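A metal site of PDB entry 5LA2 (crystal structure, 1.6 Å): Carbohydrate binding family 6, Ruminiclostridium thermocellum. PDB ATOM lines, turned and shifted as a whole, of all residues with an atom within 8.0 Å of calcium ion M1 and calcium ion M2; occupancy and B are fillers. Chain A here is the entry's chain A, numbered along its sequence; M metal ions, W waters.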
ATOM      1  N   ASN A 353      17.920  17.402 -11.321  1.00  0.00           N
ATOM      2  CA  ASN A 353      16.537  17.427 -10.867  1.00  0.00           C
ATOM      3  C   ASN A 353      15.750  16.274 -11.497  1.00  0.00           C
ATOM      4  O   ASN A 353      15.840  15.986 -12.708  1.00  0.00           O
ATOM      5  CB  ASN A 353      15.920  18.814 -11.160  1.00  0.00           C
ATOM      6  CG  ASN A 353      14.730  19.128 -10.293  1.00  0.00           C
ATOM      7  OD1 ASN A 353      14.448  18.443  -9.333  1.00  0.00           O
ATOM      8  ND2 ASN A 353      14.029  20.206 -10.637  1.00  0.00           N
ATOM      9  N   TYR A 357      18.092  14.409  -7.095  1.00  0.00           N
ATOM     10  CA  TYR A 357      17.248  15.137  -6.150  1.00  0.00           C
ATOM     11  C   TYR A 357      16.015  15.593  -6.896  1.00  0.00           C
ATOM     12  O   TYR A 357      15.967  15.539  -8.110  1.00  0.00           O
ATOM     13  CB  TYR A 357      17.990  16.355  -5.624  1.00  0.00           C
ATOM     14  CG  TYR A 357      18.349  17.371  -6.688  1.00  0.00           C
ATOM     15  CD1 TYR A 357      17.475  18.402  -7.021  1.00  0.00           C
ATOM     16  CD2 TYR A 357      19.592  17.312  -7.344  1.00  0.00           C
ATOM     17  CE1 TYR A 357      17.821  19.360  -7.985  1.00  0.00           C
ATOM     18  CE2 TYR A 357      19.946  18.267  -8.302  1.00  0.00           C
ATOM     19  CZ  TYR A 357      19.044  19.274  -8.625  1.00  0.00           C
ATOM     20  OH  TYR A 357      19.411  20.205  -9.558  1.00  0.00           O
ATOM     21  N   TYR A 358      15.041  16.077  -6.157  1.00  0.00           N
ATOM     22  CA  TYR A 358      13.952  16.836  -6.711  1.00  0.00           C
ATOM     23  C   TYR A 358      13.803  18.093  -5.860  1.00  0.00           C
ATOM     24  O   TYR A 358      13.596  18.008  -4.626  1.00  0.00           O
ATOM     25  CB  TYR A 358      12.652  16.034  -6.726  1.00  0.00           C
ATOM     26  CG  TYR A 358      11.407  16.884  -6.950  1.00  0.00           C
ATOM     27  CD1 TYR A 358      11.351  17.845  -7.971  1.00  0.00           C
ATOM     28  CD2 TYR A 358      10.306  16.729  -6.134  1.00  0.00           C
ATOM     29  CE1 TYR A 358      10.218  18.624  -8.166  1.00  0.00           C
ATOM     30  CE2 TYR A 358       9.168  17.488  -6.329  1.00  0.00           C
ATOM     31  CZ  TYR A 358       9.130  18.445  -7.325  1.00  0.00           C
ATOM     32  OH  TYR A 358       7.989  19.184  -7.506  1.00  0.00           O
ATOM     33  N   ASP A 359      13.962  19.233  -6.520  1.00  0.00           N
ATOM     34  CA  ASP A 359      13.642  20.506  -5.913  1.00  0.00           C
ATOM     35  C   ASP A 359      12.540  21.217  -6.676  1.00  0.00           C
ATOM     36  O   ASP A 359      12.506  21.149  -7.915  1.00  0.00           O
ATOM     37  CB  ASP A 359      14.887  21.395  -5.829  1.00  0.00           C
ATOM     38  CG  ASP A 359      14.784  22.349  -4.684  1.00  0.00           C
ATOM     39  OD1 ASP A 359      15.185  21.948  -3.563  1.00  0.00           O
ATOM     40  OD2 ASP A 359      14.300  23.504  -4.881  1.00  0.00           O
ATOM     41  N   THR A 360      11.666  21.892  -5.951  1.00  0.00           N
ATOM     42  CA  THR A 360      10.470  22.514  -6.567  1.00  0.00           C
ATOM     43  C   THR A 360      10.762  23.733  -7.431  1.00  0.00           C
ATOM     44  O   THR A 360       9.939  24.091  -8.270  1.00  0.00           O
ATOM     45  CB  THR A 360       9.431  22.941  -5.518  1.00  0.00           C
ATOM     46  OG1 THR A 360      10.020  23.898  -4.621  1.00  0.00           O
ATOM     47  CG2 THR A 360       8.905  21.723  -4.766  1.00  0.00           C
ATOM     48  N   ASP A 361      11.911  24.358  -7.243  1.00  0.00           N
ATOM     49  CA  ASP A 361      12.371  25.439  -8.127  1.00  0.00           C
ATOM     50  C   ASP A 361      13.818  25.211  -8.501  1.00  0.00           C
ATOM     51  O   ASP A 361      14.610  24.768  -7.668  1.00  0.00           O
ATOM     52  CB  ASP A 361      12.097  26.866  -7.577  1.00  0.00           C
ATOM     53  CG  ASP A 361      12.440  27.047  -6.097  1.00  0.00           C
ATOM     54  OD1 ASP A 361      13.441  26.499  -5.604  1.00  0.00           O
ATOM     55  OD2 ASP A 361      11.706  27.799  -5.411  1.00  0.00           O
ATOM     56  N   SER A 362      14.171  25.494  -9.756  1.00  0.00           N
ATOM     57  CA  SER A 362      15.512  25.180 -10.225  1.00  0.00           C
ATOM     58  C   SER A 362      16.551  26.184  -9.714  1.00  0.00           C
ATOM     59  O   SER A 362      17.727  25.881  -9.697  1.00  0.00           O
ATOM     60  CB  SER A 362      15.548  25.105 -11.733  1.00  0.00           C
ATOM     61  OG  SER A 362      15.127  26.316 -12.253  1.00  0.00           O
ATOM     62  N   VAL A 363      16.136  27.370  -9.304  1.00  0.00           N
ATOM     63  CA  VAL A 363      17.074  28.265  -8.610  1.00  0.00           C
ATOM     64  C   VAL A 363      17.521  27.644  -7.271  1.00  0.00           C
ATOM     65  O   VAL A 363      16.752  26.946  -6.620  1.00  0.00           O
ATOM     66  CB  VAL A 363      16.438  29.665  -8.391  1.00  0.00           C
ATOM     67  CG1 VAL A 363      15.312  29.620  -7.379  1.00  0.00           C
ATOM     68  CG2 VAL A 363      17.499  30.695  -8.004  1.00  0.00           C
ATOM     69  N   ASN A 364      18.778  27.855  -6.898  1.00  0.00           N
ATOM     70  CA  ASN A 364      19.236  27.603  -5.543  1.00  0.00           C
ATOM     71  C   ASN A 364      19.007  28.903  -4.755  1.00  0.00           C
ATOM     72  O   ASN A 364      19.807  29.838  -4.826  1.00  0.00           O
ATOM     73  CB  ASN A 364      20.702  27.202  -5.591  1.00  0.00           C
ATOM     74  CG  ASN A 364      21.335  27.090  -4.214  1.00  0.00           C
ATOM     75  OD1 ASN A 364      20.760  27.497  -3.198  1.00  0.00           O
ATOM     76  ND2 ASN A 364      22.537  26.572  -4.190  1.00  0.00           N
ATOM     77  N   VAL A 365      17.935  28.968  -3.983  1.00  0.00           N
ATOM     78  CA  VAL A 365      17.508  30.280  -3.408  1.00  0.00           C
ATOM     79  C   VAL A 365      18.528  30.831  -2.399  1.00  0.00           C
ATOM     80  O   VAL A 365      18.763  32.031  -2.330  1.00  0.00           O
ATOM     81  CB  VAL A 365      16.086  30.242  -2.785  1.00  0.00           C
ATOM     82  CG1 VAL A 365      15.035  29.709  -3.744  1.00  0.00           C
ATOM     83  CG2 VAL A 365      16.058  29.396  -1.573  1.00  0.00           C
ATOM     84  N   GLY A 366      19.161  29.945  -1.633  1.00  0.00           N
ATOM     85  CA  GLY A 366      20.240  30.347  -0.741  1.00  0.00           C
ATOM     86  C   GLY A 366      21.501  30.790  -1.462  1.00  0.00           C
ATOM     87  O   GLY A 366      22.292  31.560  -0.908  1.00  0.00           O
ATOM     88  N   GLU A 373      22.845  23.956  -9.240  1.00  0.00           N
ATOM     89  CA  GLU A 373      21.815  22.936  -9.043  1.00  0.00           C
ATOM     90  C   GLU A 373      20.653  23.501  -8.226  1.00  0.00           C
ATOM     91  O   GLU A 373      20.727  24.586  -7.670  1.00  0.00           O
ATOM     92  CB  GLU A 373      22.425  21.705  -8.390  1.00  0.00           C
ATOM     93  CG  GLU A 373      23.398  21.004  -9.312  1.00  0.00           C
ATOM     94  CD  GLU A 373      24.427  20.199  -8.570  1.00  0.00           C
ATOM     95  OE1 GLU A 373      25.416  20.792  -8.057  1.00  0.00           O
ATOM     96  OE2 GLU A 373      24.253  18.972  -8.507  1.00  0.00           O
ATOM     97  N   GLY A 374      19.552  22.770  -8.190  1.00  0.00           N
ATOM     98  CA  GLY A 374      18.304  23.297  -7.683  1.00  0.00           C
ATOM     99  C   GLY A 374      18.075  23.217  -6.194  1.00  0.00           C
ATOM    100  O   GLY A 374      17.158  23.842  -5.686  1.00  0.00           O
ATOM    101  N   VAL A 375      18.886  22.429  -5.495  1.00  0.00           N
ATOM    102  CA  VAL A 375      18.715  22.292  -4.054  1.00  0.00           C
ATOM    103  C   VAL A 375      19.040  23.651  -3.411  1.00  0.00           C
ATOM    104  O   VAL A 375      19.960  24.339  -3.821  1.00  0.00           O
ATOM    105  CB  VAL A 375      19.597  21.175  -3.504  1.00  0.00           C
ATOM    106  CG1 VAL A 375      19.477  21.065  -1.984  1.00  0.00           C
ATOM    107  CG2 VAL A 375      19.244  19.864  -4.212  1.00  0.00           C
ATOM    108  N   ASP A 376      18.249  24.044  -2.418  1.00  0.00           N
ATOM    109  CA  ASP A 376      18.423  25.351  -1.796  1.00  0.00           C
ATOM    110  C   ASP A 376      19.362  25.230  -0.613  1.00  0.00           C
ATOM    111  O   ASP A 376      19.052  24.501   0.335  1.00  0.00           O
ATOM    112  CB  ASP A 376      17.055  25.921  -1.404  1.00  0.00           C
ATOM    113  CG  ASP A 376      16.115  25.928  -2.593  1.00  0.00           C
ATOM    114  OD1 ASP A 376      16.544  26.460  -3.669  1.00  0.00           O
ATOM    115  OD2 ASP A 376      15.020  25.309  -2.524  1.00  0.00           O
ATOM    116  N   ILE A 377      20.495  25.932  -0.720  1.00  0.00           N
ATOM    117  CA  ILE A 377      21.597  25.800   0.185  1.00  0.00           C
ATOM    118  C   ILE A 377      22.073  27.161   0.711  1.00  0.00           C
ATOM    119  O   ILE A 377      22.331  28.069  -0.084  1.00  0.00           O
ATOM    120  CB  ILE A 377      22.789  25.061  -0.444  1.00  0.00           C
ATOM    121  CG1 ILE A 377      22.362  23.739  -1.090  1.00  0.00           C
ATOM    122  CG2 ILE A 377      23.814  24.721   0.629  1.00  0.00           C
ATOM    123  CD1 ILE A 377      23.453  23.079  -1.915  1.00  0.00           C
ATOM    124  N   VAL A 389      20.935  22.504   3.879  1.00  0.00           N
ATOM    125  CA  VAL A 389      19.863  22.566   2.959  1.00  0.00           C
ATOM    126  C   VAL A 389      18.677  23.221   3.669  1.00  0.00           C
ATOM    127  O   VAL A 389      18.347  22.880   4.804  1.00  0.00           O
ATOM    128  CB  VAL A 389      19.473  21.151   2.453  1.00  0.00           C
ATOM    129  CG1 VAL A 389      18.239  21.256   1.560  1.00  0.00           C
ATOM    130  CG2 VAL A 389      20.652  20.519   1.708  1.00  0.00           C
ATOM    131  N   GLY A 390      18.058  24.165   2.975  1.00  0.00           N
ATOM    132  CA  GLY A 390      16.947  24.935   3.472  1.00  0.00           C
ATOM    133  C   GLY A 390      15.868  25.000   2.423  1.00  0.00           C
ATOM    134  O   GLY A 390      15.998  24.411   1.341  1.00  0.00           O
ATOM    135  N   TRP A 391      14.820  25.754   2.707  1.00  0.00           N
ATOM    136  CA  TRP A 391      13.649  25.842   1.775  1.00  0.00           C
ATOM    137  C   TRP A 391      13.259  24.458   1.264  1.00  0.00           C
ATOM    138  O   TRP A 391      13.185  24.214   0.066  1.00  0.00           O
ATOM    139  CB  TRP A 391      13.928  26.756   0.576  1.00  0.00           C
ATOM    140  CG  TRP A 391      14.300  28.135   0.990  1.00  0.00           C
ATOM    141  CD1 TRP A 391      13.476  29.203   1.102  1.00  0.00           C
ATOM    142  CD2 TRP A 391      15.621  28.599   1.350  1.00  0.00           C
ATOM    143  NE1 TRP A 391      14.199  30.313   1.475  1.00  0.00           N
ATOM    144  CE2 TRP A 391      15.516  29.961   1.647  1.00  0.00           C
ATOM    145  CE3 TRP A 391      16.874  27.996   1.413  1.00  0.00           C
ATOM    146  CZ2 TRP A 391      16.627  30.729   2.041  1.00  0.00           C
ATOM    147  CZ3 TRP A 391      17.978  28.745   1.793  1.00  0.00           C
ATOM    148  CH2 TRP A 391      17.845  30.104   2.109  1.00  0.00           C
ATOM    149  N   ILE A 392      13.082  23.549   2.188  1.00  0.00           N
ATOM    150  CA  ILE A 392      12.701  22.183   1.877  1.00  0.00           C
ATOM    151  C   ILE A 392      11.183  22.215   1.844  1.00  0.00           C
ATOM    152  O   ILE A 392      10.561  22.563   2.851  1.00  0.00           O
ATOM    153  CB  ILE A 392      13.201  21.196   2.925  1.00  0.00           C
ATOM    154  CG1 ILE A 392      14.727  21.234   3.024  1.00  0.00           C
ATOM    155  CG2 ILE A 392      12.726  19.782   2.569  1.00  0.00           C
ATOM    156  CD1 ILE A 392      15.315  20.193   3.984  1.00  0.00           C
ATOM    157  N   SER A 393      10.644  21.867   0.689  1.00  0.00           N
ATOM    158  CA  SER A 393       9.214  21.856   0.418  1.00  0.00           C
ATOM    159  C   SER A 393       8.664  20.440   0.318  1.00  0.00           C
ATOM    160  O   SER A 393       9.357  19.502  -0.068  1.00  0.00           O
ATOM    161  CB  SER A 393       8.977  22.577  -0.893  1.00  0.00           C
ATOM    162  OG  SER A 393       9.494  23.898  -0.750  1.00  0.00           O
ATOM    163  N   GLU A 394       7.391  20.313   0.654  1.00  0.00           N
ATOM    164  CA  GLU A 394       6.688  19.051   0.593  1.00  0.00           C
ATOM    165  C   GLU A 394       6.902  18.379  -0.771  1.00  0.00           C
ATOM    166  O   GLU A 394       6.797  19.033  -1.820  1.00  0.00           O
ATOM    167  CB  GLU A 394       5.202  19.312   0.860  1.00  0.00           C
ATOM    168  CG  GLU A 394       4.339  18.072   0.869  1.00  0.00           C
ATOM    169  CD  GLU A 394       2.862  18.383   0.901  1.00  0.00           C
ATOM    170  OE1 GLU A 394       2.465  19.575   0.893  1.00  0.00           O
ATOM    171  OE2 GLU A 394       2.090  17.409   0.937  1.00  0.00           O
ATOM    172  N   GLU A 396       9.800  17.208  -1.941  1.00  0.00           N
ATOM    173  CA  GLU A 396      11.196  17.220  -2.296  1.00  0.00           C
ATOM    174  C   GLU A 396      11.910  15.951  -1.798  1.00  0.00           C
ATOM    175  O   GLU A 396      11.466  15.258  -0.862  1.00  0.00           O
ATOM    176  CB  GLU A 396      11.863  18.500  -1.784  1.00  0.00           C
ATOM    177  CG  GLU A 396      11.440  19.703  -2.598  1.00  0.00           C
ATOM    178  CD  GLU A 396      12.223  20.962  -2.320  1.00  0.00           C
ATOM    179  OE1 GLU A 396      12.858  21.109  -1.247  1.00  0.00           O
ATOM    180  OE2 GLU A 396      12.222  21.835  -3.189  1.00  0.00           O
ATOM    181  N   TRP A 397      13.006  15.631  -2.471  1.00  0.00           N
ATOM    182  CA  TRP A 397      13.863  14.532  -2.052  1.00  0.00           C
ATOM    183  C   TRP A 397      15.312  14.737  -2.478  1.00  0.00           C
ATOM    184  O   TRP A 397      15.601  15.533  -3.354  1.00  0.00           O
ATOM    185  CB  TRP A 397      13.322  13.188  -2.552  1.00  0.00           C
ATOM    186  CG  TRP A 397      12.946  13.077  -3.981  1.00  0.00           C
ATOM    187  CD1 TRP A 397      11.690  13.248  -4.508  1.00  0.00           C
ATOM    188  CD2 TRP A 397      13.791  12.680  -5.083  1.00  0.00           C
ATOM    189  NE1 TRP A 397      11.707  12.991  -5.849  1.00  0.00           N
ATOM    190  CE2 TRP A 397      12.989  12.650  -6.231  1.00  0.00           C
ATOM    191  CE3 TRP A 397      15.141  12.331  -5.196  1.00  0.00           C
ATOM    192  CZ2 TRP A 397      13.477  12.288  -7.474  1.00  0.00           C
ATOM    193  CZ3 TRP A 397      15.633  11.998  -6.417  1.00  0.00           C
ATOM    194  CH2 TRP A 397      14.804  11.976  -7.561  1.00  0.00           C
ATOM    195  N   LEU A 398      16.198  14.052  -1.757  1.00  0.00           N
ATOM    196  CA  LEU A 398      17.643  14.134  -1.894  1.00  0.00           C
ATOM    197  C   LEU A 398      18.212  12.729  -1.766  1.00  0.00           C
ATOM    198  O   LEU A 398      17.823  11.960  -0.865  1.00  0.00           O
ATOM    199  CB  LEU A 398      18.233  14.954  -0.739  1.00  0.00           C
ATOM    200  CG  LEU A 398      17.712  16.366  -0.602  1.00  0.00           C
ATOM    201  CD1 LEU A 398      17.851  16.871   0.827  1.00  0.00           C
ATOM    202  CD2 LEU A 398      18.418  17.269  -1.591  1.00  0.00           C
HETATM  203 CA    CA M   1      13.829  23.369  -2.100  1.00  0.00          CA
HETATM  204 CA    CA M   2      15.431  25.409  -5.511  1.00  0.00          CA
HETATM  205  O   HOH W   1      11.814  24.653  -2.638  1.00  0.00           O
HETATM  206  O   HOH W   2      15.865  22.759  -0.860  1.00  0.00           O
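Of the 25 residues printed, 5 come within 4 Å of calcium ion M2.
The backbone NH (N) of Asp 359 sits at hydrogen-bond distance from the side-chain amide oxygen (OD1) of Asn 353, 3.0 Å away. The backbone NH (N) of Gly 390 sits at hydrogen-bond distance from the backbone carbonyl oxygen (O) of Asp 376 (2.8 Å). OD1 of Asp 376 lies close to N of Val 365, 2.9 Å away. OH of Tyr 357 is in hydrogen-bond range of N of Gly 374. OE1 of Glu 396 sits close to N of Ser 393, 3.0 Å away. The side-chain carboxylate (OE2) of Glu 396 sits close to the backbone NH (N) of Thr 360, 2.8 Å away.
Water W2 bridges the backbone carbonyl oxygen of Gly 390 (2.8 Å) and the backbone NH of Asp 376 (3.1 Å). Water W1 lies within hydrogen-bond range of the side-chain hydroxyl of Thr 360 (2.8 Å) and the side-chain hydroxyl of Ser 393 (3.1 Å).
Of the 25 residues printed, 4 come within 4 Å of calcium ion M1.
Calcium ion M1 is bound by the side-chain carboxylate (OD2) of Asp 376. Calcium ion M1 is bound by the backbone carbonyl oxygen (O) of Trp 391 (2.4 Å). OD1 of Asp 359 binds calcium ion M1 (2.4 Å). Water W1 binds calcium ion M1. Water W2 is bound to calcium ion M1 (2.5 Å). Calcium ion M1 is bound by OE2 of Glu 396 (2.5 Å). OE1 of Glu 396 binds calcium ion M1, 2.6 Å away. Calcium ion M1 is bound by OD2 of Asp 359 (2.8 Å). Calcium ion M1 has eight donor atoms within binding distance.
Calcium ion M2 is bound by the side-chain carboxylate (OD1) of Asp 361 (2.3 Å), the side-chain carboxylate (OD2) of Asp 359 (2.3 Å), the backbone carbonyl oxygen (O) of Val 363 (2.3 Å), the backbone carbonyl oxygen (O) of Gly 374 (2.3 Å), the backbone carbonyl oxygen (O) of Asp 361 (2.4 Å) and the side-chain carboxylate (OD1) of Asp 376 (2.4 Å). Slightly farther from calcium ion M2 lies the side-chain carboxylate (OD2) of Asp 376 (3.0 Å).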
